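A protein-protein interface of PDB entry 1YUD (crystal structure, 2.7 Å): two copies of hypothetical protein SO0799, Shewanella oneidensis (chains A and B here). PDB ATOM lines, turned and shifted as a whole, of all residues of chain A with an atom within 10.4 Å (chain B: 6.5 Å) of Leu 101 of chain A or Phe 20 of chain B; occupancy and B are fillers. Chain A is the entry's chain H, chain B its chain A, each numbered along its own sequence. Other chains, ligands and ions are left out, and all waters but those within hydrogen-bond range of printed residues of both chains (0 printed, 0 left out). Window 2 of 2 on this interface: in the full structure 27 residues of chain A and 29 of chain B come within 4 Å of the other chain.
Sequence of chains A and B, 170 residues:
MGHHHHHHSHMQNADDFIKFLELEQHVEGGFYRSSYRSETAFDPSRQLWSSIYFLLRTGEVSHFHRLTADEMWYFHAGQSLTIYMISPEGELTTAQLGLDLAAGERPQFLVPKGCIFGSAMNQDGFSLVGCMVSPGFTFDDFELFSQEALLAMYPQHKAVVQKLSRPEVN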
ATOM      1  N   PHE A  75       9.766  14.310 -12.738  1.00  0.00           N
ATOM      2  CA  PHE A  75       9.566  14.859 -14.072  1.00  0.00           C
ATOM      3  C   PHE A  75      10.882  14.974 -14.832  1.00  0.00           C
ATOM      4  O   PHE A  75      11.805  15.640 -14.359  1.00  0.00           O
ATOM      5  CB  PHE A  75       8.970  16.243 -14.043  1.00  0.00           C
ATOM      6  CG  PHE A  75       8.779  16.826 -15.411  1.00  0.00           C
ATOM      7  CD1 PHE A  75       7.592  16.619 -16.099  1.00  0.00           C
ATOM      8  CD2 PHE A  75       9.791  17.594 -16.010  1.00  0.00           C
ATOM      9  CE1 PHE A  75       7.394  17.173 -17.372  1.00  0.00           C
ATOM     10  CE2 PHE A  75       9.613  18.156 -17.287  1.00  0.00           C
ATOM     11  CZ  PHE A  75       8.407  17.944 -17.964  1.00  0.00           C
ATOM     12  N   SER A  80       3.743  18.903 -19.017  1.00  0.00           N
ATOM     13  CA  SER A  80       3.490  18.585 -17.615  1.00  0.00           C
ATOM     14  C   SER A  80       2.252  17.689 -17.523  1.00  0.00           C
ATOM     15  O   SER A  80       1.391  17.685 -18.427  1.00  0.00           O
ATOM     16  CB  SER A  80       3.317  19.863 -16.755  1.00  0.00           C
ATOM     17  OG  SER A  80       2.334  20.762 -17.251  1.00  0.00           O
ATOM     18  N   GLN A  96       0.141  18.018  -9.778  1.00  0.00           N
ATOM     19  CA  GLN A  96       0.619  18.242 -11.122  1.00  0.00           C
ATOM     20  C   GLN A  96       2.112  18.102 -11.050  1.00  0.00           C
ATOM     21  O   GLN A  96       2.729  18.515 -10.069  1.00  0.00           O
ATOM     22  CB  GLN A  96       0.181  19.608 -11.603  1.00  0.00           C
ATOM     23  CG  GLN A  96      -1.273  19.817 -11.288  1.00  0.00           C
ATOM     24  CD  GLN A  96      -2.004  20.609 -12.333  1.00  0.00           C
ATOM     25  OE1 GLN A  96      -2.085  20.203 -13.496  1.00  0.00           O
ATOM     26  NE2 GLN A  96      -2.556  21.754 -11.927  1.00  0.00           N
ATOM     27  N   LEU A  97       2.689  17.467 -12.062  1.00  0.00           N
ATOM     28  CA  LEU A  97       4.122  17.249 -12.085  1.00  0.00           C
ATOM     29  C   LEU A  97       4.661  18.073 -13.229  1.00  0.00           C
ATOM     30  O   LEU A  97       4.036  18.134 -14.292  1.00  0.00           O
ATOM     31  CB  LEU A  97       4.412  15.773 -12.318  1.00  0.00           C
ATOM     32  CG  LEU A  97       5.827  15.296 -12.017  1.00  0.00           C
ATOM     33  CD1 LEU A  97       5.960  15.074 -10.524  1.00  0.00           C
ATOM     34  CD2 LEU A  97       6.130  14.013 -12.777  1.00  0.00           C
ATOM     35  N   GLY A  98       5.801  18.718 -13.015  1.00  0.00           N
ATOM     36  CA  GLY A  98       6.386  19.544 -14.059  1.00  0.00           C
ATOM     37  C   GLY A  98       7.343  20.625 -13.568  1.00  0.00           C
ATOM     38  O   GLY A  98       8.037  20.460 -12.553  1.00  0.00           O
ATOM     39  N   LEU A  99       7.376  21.751 -14.273  1.00  0.00           N
ATOM     40  CA  LEU A  99       8.286  22.826 -13.896  1.00  0.00           C
ATOM     41  C   LEU A  99       7.665  24.199 -13.639  1.00  0.00           C
ATOM     42  O   LEU A  99       8.345  25.097 -13.151  1.00  0.00           O
ATOM     43  CB  LEU A  99       9.380  22.949 -14.957  1.00  0.00           C
ATOM     44  CG  LEU A  99      10.121  21.638 -15.222  1.00  0.00           C
ATOM     45  CD1 LEU A  99      11.177  21.833 -16.314  1.00  0.00           C
ATOM     46  CD2 LEU A  99      10.752  21.163 -13.935  1.00  0.00           C
ATOM     47  N   ASP A 100       6.389  24.367 -13.968  1.00  0.00           N
ATOM     48  CA  ASP A 100       5.703  25.638 -13.760  1.00  0.00           C
ATOM     49  C   ASP A 100       5.362  25.810 -12.271  1.00  0.00           C
ATOM     50  O   ASP A 100       4.206  25.689 -11.862  1.00  0.00           O
ATOM     51  CB  ASP A 100       4.440  25.674 -14.626  1.00  0.00           C
ATOM     52  CG  ASP A 100       3.692  26.996 -14.534  1.00  0.00           C
ATOM     53  OD1 ASP A 100       3.010  27.348 -15.524  1.00  0.00           O
ATOM     54  OD2 ASP A 100       3.770  27.673 -13.480  1.00  0.00           O
ATOM     55  N   LEU A 101       6.393  26.107 -11.483  1.00  0.00           N
ATOM     56  CA  LEU A 101       6.296  26.290 -10.034  1.00  0.00           C
ATOM     57  C   LEU A 101       5.273  27.342  -9.594  1.00  0.00           C
ATOM     58  O   LEU A 101       4.806  27.317  -8.450  1.00  0.00           O
ATOM     59  CB  LEU A 101       7.685  26.631  -9.488  1.00  0.00           C
ATOM     60  CG  LEU A 101       8.773  25.622  -9.901  1.00  0.00           C
ATOM     61  CD1 LEU A 101      10.124  26.324 -10.115  1.00  0.00           C
ATOM     62  CD2 LEU A 101       8.867  24.515  -8.853  1.00  0.00           C
ATOM     63  N   ALA A 102       4.933  28.259 -10.504  1.00  0.00           N
ATOM     64  CA  ALA A 102       3.946  29.316 -10.231  1.00  0.00           C
ATOM     65  C   ALA A 102       2.619  28.660  -9.858  1.00  0.00           C
ATOM     66  O   ALA A 102       1.921  29.106  -8.948  1.00  0.00           O
ATOM     67  CB  ALA A 102       3.761  30.200 -11.459  1.00  0.00           C
ATOM     68  N   ALA A 103       2.263  27.607 -10.586  1.00  0.00           N
ATOM     69  CA  ALA A 103       1.049  26.874 -10.280  1.00  0.00           C
ATOM     70  C   ALA A 103       1.505  25.775  -9.326  1.00  0.00           C
ATOM     71  O   ALA A 103       2.655  25.778  -8.873  1.00  0.00           O
ATOM     72  CB  ALA A 103       0.458  26.278 -11.534  1.00  0.00           C
ATOM     73  N   GLY A 104       0.621  24.834  -9.016  1.00  0.00           N
ATOM     74  CA  GLY A 104       1.004  23.772  -8.100  1.00  0.00           C
ATOM     75  C   GLY A 104       1.935  22.746  -8.716  1.00  0.00           C
ATOM     76  O   GLY A 104       2.069  21.636  -8.187  1.00  0.00           O
ATOM     77  N   GLU A 105       2.574  23.099  -9.831  1.00  0.00           N
ATOM     78  CA  GLU A 105       3.479  22.175 -10.506  1.00  0.00           C
ATOM     79  C   GLU A 105       4.781  21.985  -9.761  1.00  0.00           C
ATOM     80  O   GLU A 105       5.441  22.945  -9.382  1.00  0.00           O
ATOM     81  CB  GLU A 105       3.759  22.632 -11.937  1.00  0.00           C
ATOM     82  CG  GLU A 105       2.774  22.080 -12.944  1.00  0.00           C
ATOM     83  CD  GLU A 105       3.160  22.397 -14.365  1.00  0.00           C
ATOM     84  OE1 GLU A 105       4.357  22.270 -14.695  1.00  0.00           O
ATOM     85  OE2 GLU A 105       2.265  22.759 -15.154  1.00  0.00           O
ATOM     86  N   ARG A 106       5.141  20.727  -9.554  1.00  0.00           N
ATOM     87  CA  ARG A 106       6.354  20.373  -8.837  1.00  0.00           C
ATOM     88  C   ARG A 106       7.093  19.375  -9.746  1.00  0.00           C
ATOM     89  O   ARG A 106       6.460  18.657 -10.524  1.00  0.00           O
ATOM     90  CB  ARG A 106       5.967  19.724  -7.498  1.00  0.00           C
ATOM     91  CG  ARG A 106       6.881  20.020  -6.305  1.00  0.00           C
ATOM     92  CD  ARG A 106       6.506  21.318  -5.588  1.00  0.00           C
ATOM     93  NE  ARG A 106       6.616  22.494  -6.449  1.00  0.00           N
ATOM     94  CZ  ARG A 106       6.067  23.670  -6.172  1.00  0.00           C
ATOM     95  NH1 ARG A 106       5.371  23.820  -5.054  1.00  0.00           N
ATOM     96  NH2 ARG A 106       6.207  24.689  -7.012  1.00  0.00           N
ATOM     97  N   PRO A 107       8.435  19.329  -9.678  1.00  0.00           N
ATOM     98  CA  PRO A 107       9.146  18.382 -10.542  1.00  0.00           C
ATOM     99  C   PRO A 107       9.126  16.961  -9.976  1.00  0.00           C
ATOM    100  O   PRO A 107       9.539  16.010 -10.633  1.00  0.00           O
ATOM    101  CB  PRO A 107      10.568  18.954 -10.597  1.00  0.00           C
ATOM    102  CG  PRO A 107      10.412  20.374 -10.184  1.00  0.00           C
ATOM    103  CD  PRO A 107       9.381  20.288  -9.094  1.00  0.00           C
ATOM    104  N   GLN A 108       8.659  16.821  -8.746  1.00  0.00           N
ATOM    105  CA  GLN A 108       8.601  15.515  -8.110  1.00  0.00           C
ATOM    106  C   GLN A 108       7.271  15.319  -7.406  1.00  0.00           C
ATOM    107  O   GLN A 108       6.548  16.280  -7.139  1.00  0.00           O
ATOM    108  CB  GLN A 108       9.746  15.361  -7.112  1.00  0.00           C
ATOM    109  CG  GLN A 108      11.063  14.981  -7.757  1.00  0.00           C
ATOM    110  CD  GLN A 108      12.202  14.865  -6.765  1.00  0.00           C
ATOM    111  OE1 GLN A 108      12.060  14.264  -5.695  1.00  0.00           O
ATOM    112  NE2 GLN A 108      13.352  15.431  -7.125  1.00  0.00           N
ATOM    113  N   GLN B  12      12.694  30.194 -16.657  1.00  0.00           N
ATOM    114  CA  GLN B  12      13.079  30.055 -15.257  1.00  0.00           C
ATOM    115  C   GLN B  12      14.584  29.921 -15.075  1.00  0.00           C
ATOM    116  O   GLN B  12      15.292  29.457 -15.970  1.00  0.00           O
ATOM    117  CB  GLN B  12      12.391  28.833 -14.638  1.00  0.00           C
ATOM    118  CG  GLN B  12      10.992  29.084 -14.090  1.00  0.00           C
ATOM    119  CD  GLN B  12      10.386  27.845 -13.441  1.00  0.00           C
ATOM    120  OE1 GLN B  12       9.508  27.949 -12.579  1.00  0.00           O
ATOM    121  NE2 GLN B  12      10.843  26.669 -13.860  1.00  0.00           N
ATOM    122  N   ASP B  15      17.459  30.774  -9.555  1.00  0.00           N
ATOM    123  CA  ASP B  15      16.909  31.551  -8.453  1.00  0.00           C
ATOM    124  C   ASP B  15      15.468  31.181  -8.143  1.00  0.00           C
ATOM    125  O   ASP B  15      15.055  31.172  -6.982  1.00  0.00           O
ATOM    126  CB  ASP B  15      17.020  33.043  -8.768  1.00  0.00           C
ATOM    127  CG  ASP B  15      18.459  33.491  -8.928  1.00  0.00           C
ATOM    128  OD1 ASP B  15      19.253  33.277  -7.985  1.00  0.00           O
ATOM    129  OD2 ASP B  15      18.797  34.052  -9.991  1.00  0.00           O
ATOM    130  N   ASP B  16      14.709  30.870  -9.189  1.00  0.00           N
ATOM    131  CA  ASP B  16      13.309  30.488  -9.041  1.00  0.00           C
ATOM    132  C   ASP B  16      13.207  29.156  -8.329  1.00  0.00           C
ATOM    133  O   ASP B  16      12.393  28.985  -7.418  1.00  0.00           O
ATOM    134  CB  ASP B  16      12.646  30.368 -10.411  1.00  0.00           C
ATOM    135  CG  ASP B  16      12.613  31.679 -11.152  1.00  0.00           C
ATOM    136  OD1 ASP B  16      13.664  32.350 -11.222  1.00  0.00           O
ATOM    137  OD2 ASP B  16      11.537  32.038 -11.666  1.00  0.00           O
ATOM    138  N   PHE B  17      14.047  28.216  -8.754  1.00  0.00           N
ATOM    139  CA  PHE B  17      14.067  26.880  -8.177  1.00  0.00           C
ATOM    140  C   PHE B  17      14.482  26.872  -6.721  1.00  0.00           C
ATOM    141  O   PHE B  17      13.773  26.322  -5.879  1.00  0.00           O
ATOM    142  CB  PHE B  17      14.981  25.957  -8.992  1.00  0.00           C
ATOM    143  CG  PHE B  17      14.333  25.425 -10.236  1.00  0.00           C
ATOM    144  CD1 PHE B  17      14.866  25.692 -11.492  1.00  0.00           C
ATOM    145  CD2 PHE B  17      13.153  24.688 -10.151  1.00  0.00           C
ATOM    146  CE1 PHE B  17      14.229  25.237 -12.648  1.00  0.00           C
ATOM    147  CE2 PHE B  17      12.508  24.229 -11.299  1.00  0.00           C
ATOM    148  CZ  PHE B  17      13.050  24.506 -12.547  1.00  0.00           C
ATOM    149  N   ILE B  18      15.621  27.480  -6.412  1.00  0.00           N
ATOM    150  CA  ILE B  18      16.066  27.496  -5.028  1.00  0.00           C
ATOM    151  C   ILE B  18      14.984  28.113  -4.138  1.00  0.00           C
ATOM    152  O   ILE B  18      14.792  27.685  -2.995  1.00  0.00           O
ATOM    153  CB  ILE B  18      17.410  28.265  -4.864  1.00  0.00           C
ATOM    154  CG1 ILE B  18      17.269  29.705  -5.348  1.00  0.00           C
ATOM    155  CG2 ILE B  18      18.499  27.579  -5.640  1.00  0.00           C
ATOM    156  CD1 ILE B  18      16.805  30.674  -4.266  1.00  0.00           C
ATOM    157  N   LYS B  19      14.260  29.093  -4.682  1.00  0.00           N
ATOM    158  CA  LYS B  19      13.211  29.778  -3.937  1.00  0.00           C
ATOM    159  C   LYS B  19      11.953  28.937  -3.759  1.00  0.00           C
ATOM    160  O   LYS B  19      11.583  28.597  -2.635  1.00  0.00           O
ATOM    161  CB  LYS B  19      12.841  31.092  -4.623  1.00  0.00           C
ATOM    162  CG  LYS B  19      11.813  31.912  -3.838  1.00  0.00           C
ATOM    163  CD  LYS B  19      11.146  32.972  -4.708  1.00  0.00           C
ATOM    164  CE  LYS B  19      10.004  33.666  -3.968  1.00  0.00           C
ATOM    165  NZ  LYS B  19       9.206  34.563  -4.865  1.00  0.00           N
ATOM    166  N   PHE B  20      11.291  28.610  -4.866  1.00  0.00           N
ATOM    167  CA  PHE B  20      10.069  27.813  -4.808  1.00  0.00           C
ATOM    168  C   PHE B  20      10.258  26.463  -4.142  1.00  0.00           C
ATOM    169  O   PHE B  20       9.378  26.000  -3.413  1.00  0.00           O
ATOM    170  CB  PHE B  20       9.511  27.601  -6.204  1.00  0.00           C
ATOM    171  CG  PHE B  20       8.899  28.826  -6.792  1.00  0.00           C
ATOM    172  CD1 PHE B  20       7.821  29.445  -6.165  1.00  0.00           C
ATOM    173  CD2 PHE B  20       9.395  29.370  -7.973  1.00  0.00           C
ATOM    174  CE1 PHE B  20       7.243  30.585  -6.704  1.00  0.00           C
ATOM    175  CE2 PHE B  20       8.823  30.517  -8.527  1.00  0.00           C
ATOM    176  CZ  PHE B  20       7.746  31.122  -7.889  1.00  0.00           C
ATOM    177  N   LEU B  21      11.399  25.824  -4.396  1.00  0.00           N
ATOM    178  CA  LEU B  21      11.672  24.523  -3.802  1.00  0.00           C
ATOM    179  C   LEU B  21      12.412  24.646  -2.471  1.00  0.00           C
ATOM    180  O   LEU B  21      12.727  23.642  -1.837  1.00  0.00           O
ATOM    181  CB  LEU B  21      12.468  23.647  -4.773  1.00  0.00           C
ATOM    182  CG  LEU B  21      11.844  23.338  -6.142  1.00  0.00           C
ATOM    183  CD1 LEU B  21      12.810  22.481  -6.957  1.00  0.00           C
ATOM    184  CD2 LEU B  21      10.512  22.628  -5.974  1.00  0.00           C
ATOM    185  N   GLU B  22      12.688  25.881  -2.054  1.00  0.00           N
ATOM    186  CA  GLU B  22      13.356  26.148  -0.774  1.00  0.00           C
ATOM    187  C   GLU B  22      14.676  25.405  -0.609  1.00  0.00           C
ATOM    188  O   GLU B  22      14.873  24.711   0.387  1.00  0.00           O
ATOM    189  CB  GLU B  22      12.434  25.762   0.389  1.00  0.00           C
ATOM    190  CG  GLU B  22      11.024  26.318   0.292  1.00  0.00           C
ATOM    191  CD  GLU B  22      10.106  25.751   1.358  1.00  0.00           C
ATOM    192  OE1 GLU B  22       8.899  26.048   1.316  1.00  0.00           O
ATOM    193  OE2 GLU B  22      10.587  25.010   2.239  1.00  0.00           O
ATOM    194  N   LEU B  23      15.580  25.580  -1.566  1.00  0.00           N
ATOM    195  CA  LEU B  23      16.874  24.900  -1.551  1.00  0.00           C
ATOM    196  C   LEU B  23      17.980  25.560  -0.715  1.00  0.00           C
ATOM    197  O   LEU B  23      18.354  26.700  -0.951  1.00  0.00           O
ATOM    198  CB  LEU B  23      17.343  24.719  -2.994  1.00  0.00           C
ATOM    199  CG  LEU B  23      16.290  24.014  -3.857  1.00  0.00           C
ATOM    200  CD1 LEU B  23      16.632  24.127  -5.340  1.00  0.00           C
ATOM    201  CD2 LEU B  23      16.190  22.561  -3.401  1.00  0.00           C
ATOM    202  N   TYR B  53      15.841  17.306  -3.821  1.00  0.00           N
ATOM    203  CA  TYR B  53      16.022  18.035  -5.050  1.00  0.00           C
ATOM    204  C   TYR B  53      17.519  18.356  -4.951  1.00  0.00           C
ATOM    205  O   TYR B  53      18.129  18.100  -3.911  1.00  0.00           O
ATOM    206  CB  TYR B  53      15.191  19.300  -5.010  1.00  0.00           C
ATOM    207  CG  TYR B  53      13.726  19.108  -5.300  1.00  0.00           C
ATOM    208  CD1 TYR B  53      13.279  18.960  -6.612  1.00  0.00           C
ATOM    209  CD2 TYR B  53      12.775  19.148  -4.286  1.00  0.00           C
ATOM    210  CE1 TYR B  53      11.918  18.869  -6.912  1.00  0.00           C
ATOM    211  CE2 TYR B  53      11.410  19.060  -4.574  1.00  0.00           C
ATOM    212  CZ  TYR B  53      10.993  18.925  -5.886  1.00  0.00           C
ATOM    213  OH  TYR B  53       9.658  18.887  -6.206  1.00  0.00           O
ATOM    214  N   LEU B 128      18.666  21.321 -12.160  1.00  0.00           N
ATOM    215  CA  LEU B 128      17.806  20.758 -11.133  1.00  0.00           C
ATOM    216  C   LEU B 128      17.924  19.255 -11.364  1.00  0.00           C
ATOM    217  O   LEU B 128      17.854  18.779 -12.503  1.00  0.00           O
ATOM    218  CB  LEU B 128      16.353  21.205 -11.325  1.00  0.00           C
ATOM    219  CG  LEU B 128      15.455  20.646 -10.215  1.00  0.00           C
ATOM    220  CD1 LEU B 128      15.880  21.262  -8.906  1.00  0.00           C
ATOM    221  CD2 LEU B 128      13.988  20.925 -10.492  1.00  0.00           C
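The backbone carbonyl oxygen (O) of Pro 107 of chain A lies within hydrogen-bond range of the backbone NH (N) of Phe 75 of chain A (2.7 Å).
O of Gln 96 of chain A is in hydrogen-bond range of N of Arg 106 of chain A (3.3 Å).
N of Gly 98 of chain A sits at hydrogen-bond distance from O of Arg 106 of chain A, at 2.6 Å.
The backbone NH of Leu 99 of chain A lies within hydrogen-bond range of the side-chain carboxylate of Glu 105 of chain A, 3.1 Å away.
O of Leu 101 of chain A lies close to NH2 of Arg 106 of chain A (3.3 Å).
Of the printed residues of chain B, Arg 106 of chain A touches Leu 21 and Tyr 53.
Of the printed residues of chain B, Pro 107 of chain A touches Tyr 53 (3.2 Å) and Leu 128 (3.6 Å).
Asp 15 of chain B touches none of the printed residues of chain A.
Phe 17 of chain B touches one residue of chain A.
No residue of chain A comes within 4 Å of Lys 19 of chain B.
Phe 20 of chain B touches just one residue of chain A: Leu 101 (3.6 Å).
Leu 23 of chain B touches none of the printed residues of chain A.
Of the printed residues of chain A, Tyr 53 of chain B touches Arg 106, Pro 107 and Gln 108.
The nearest residue of chain A that does not touch Phe 20 of chain B is Arg 106 of chain A (4.5 Å).
Of the 15 printed residues of chain A, 5 touch a printed residue of chain B.
Of the 12 printed residues of chain B, 6 touch a printed residue of chain A.
Hydrophobic or aromatic side chains of chain B within 4 Å of the printed part of chain A: Phe 17, Phe 20, Leu 21, Tyr 53 and Leu 128.
Among the printed residues, no Asp or Glu carboxylate lies within 4 Å of a Lys or Arg side-chain nitrogen of the other chain.
The side-chain amide nitrogen of Gln 12 of chain B sits at hydrogen-bond distance from the backbone carbonyl oxygen of Leu 99 of chain A, 3.0 Å away.
The side-chain hydroxyl (OH) of Tyr 53 of chain B sits at hydrogen-bond distance from the backbone NH (N) of Gln 108 of chain A (3.4 Å).
No position is printed for both chains.
CD1 of Leu 101 of chain A touches OE1 of Gln 12 of chain B (3.0 Å).
Leu 101 of chain A touches Phe 17 of chain B (CD1 to CE2, 3.4 Å).
CB of Leu 101 of chain A touches CD2 of Phe 20 of chain B (3.6 Å).
Leu 101 of chain A touches Leu 21 of chain B.
Arg 106 of chain A touches Leu 21 of chain B.
Arg 106 of chain A touches Tyr 53 of chain B.
OH of Tyr 53 of chain B touches CD of Pro 107 of chain A, at 3.2 Å.
Pro 107 of chain A touches Leu 128 of chain B.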
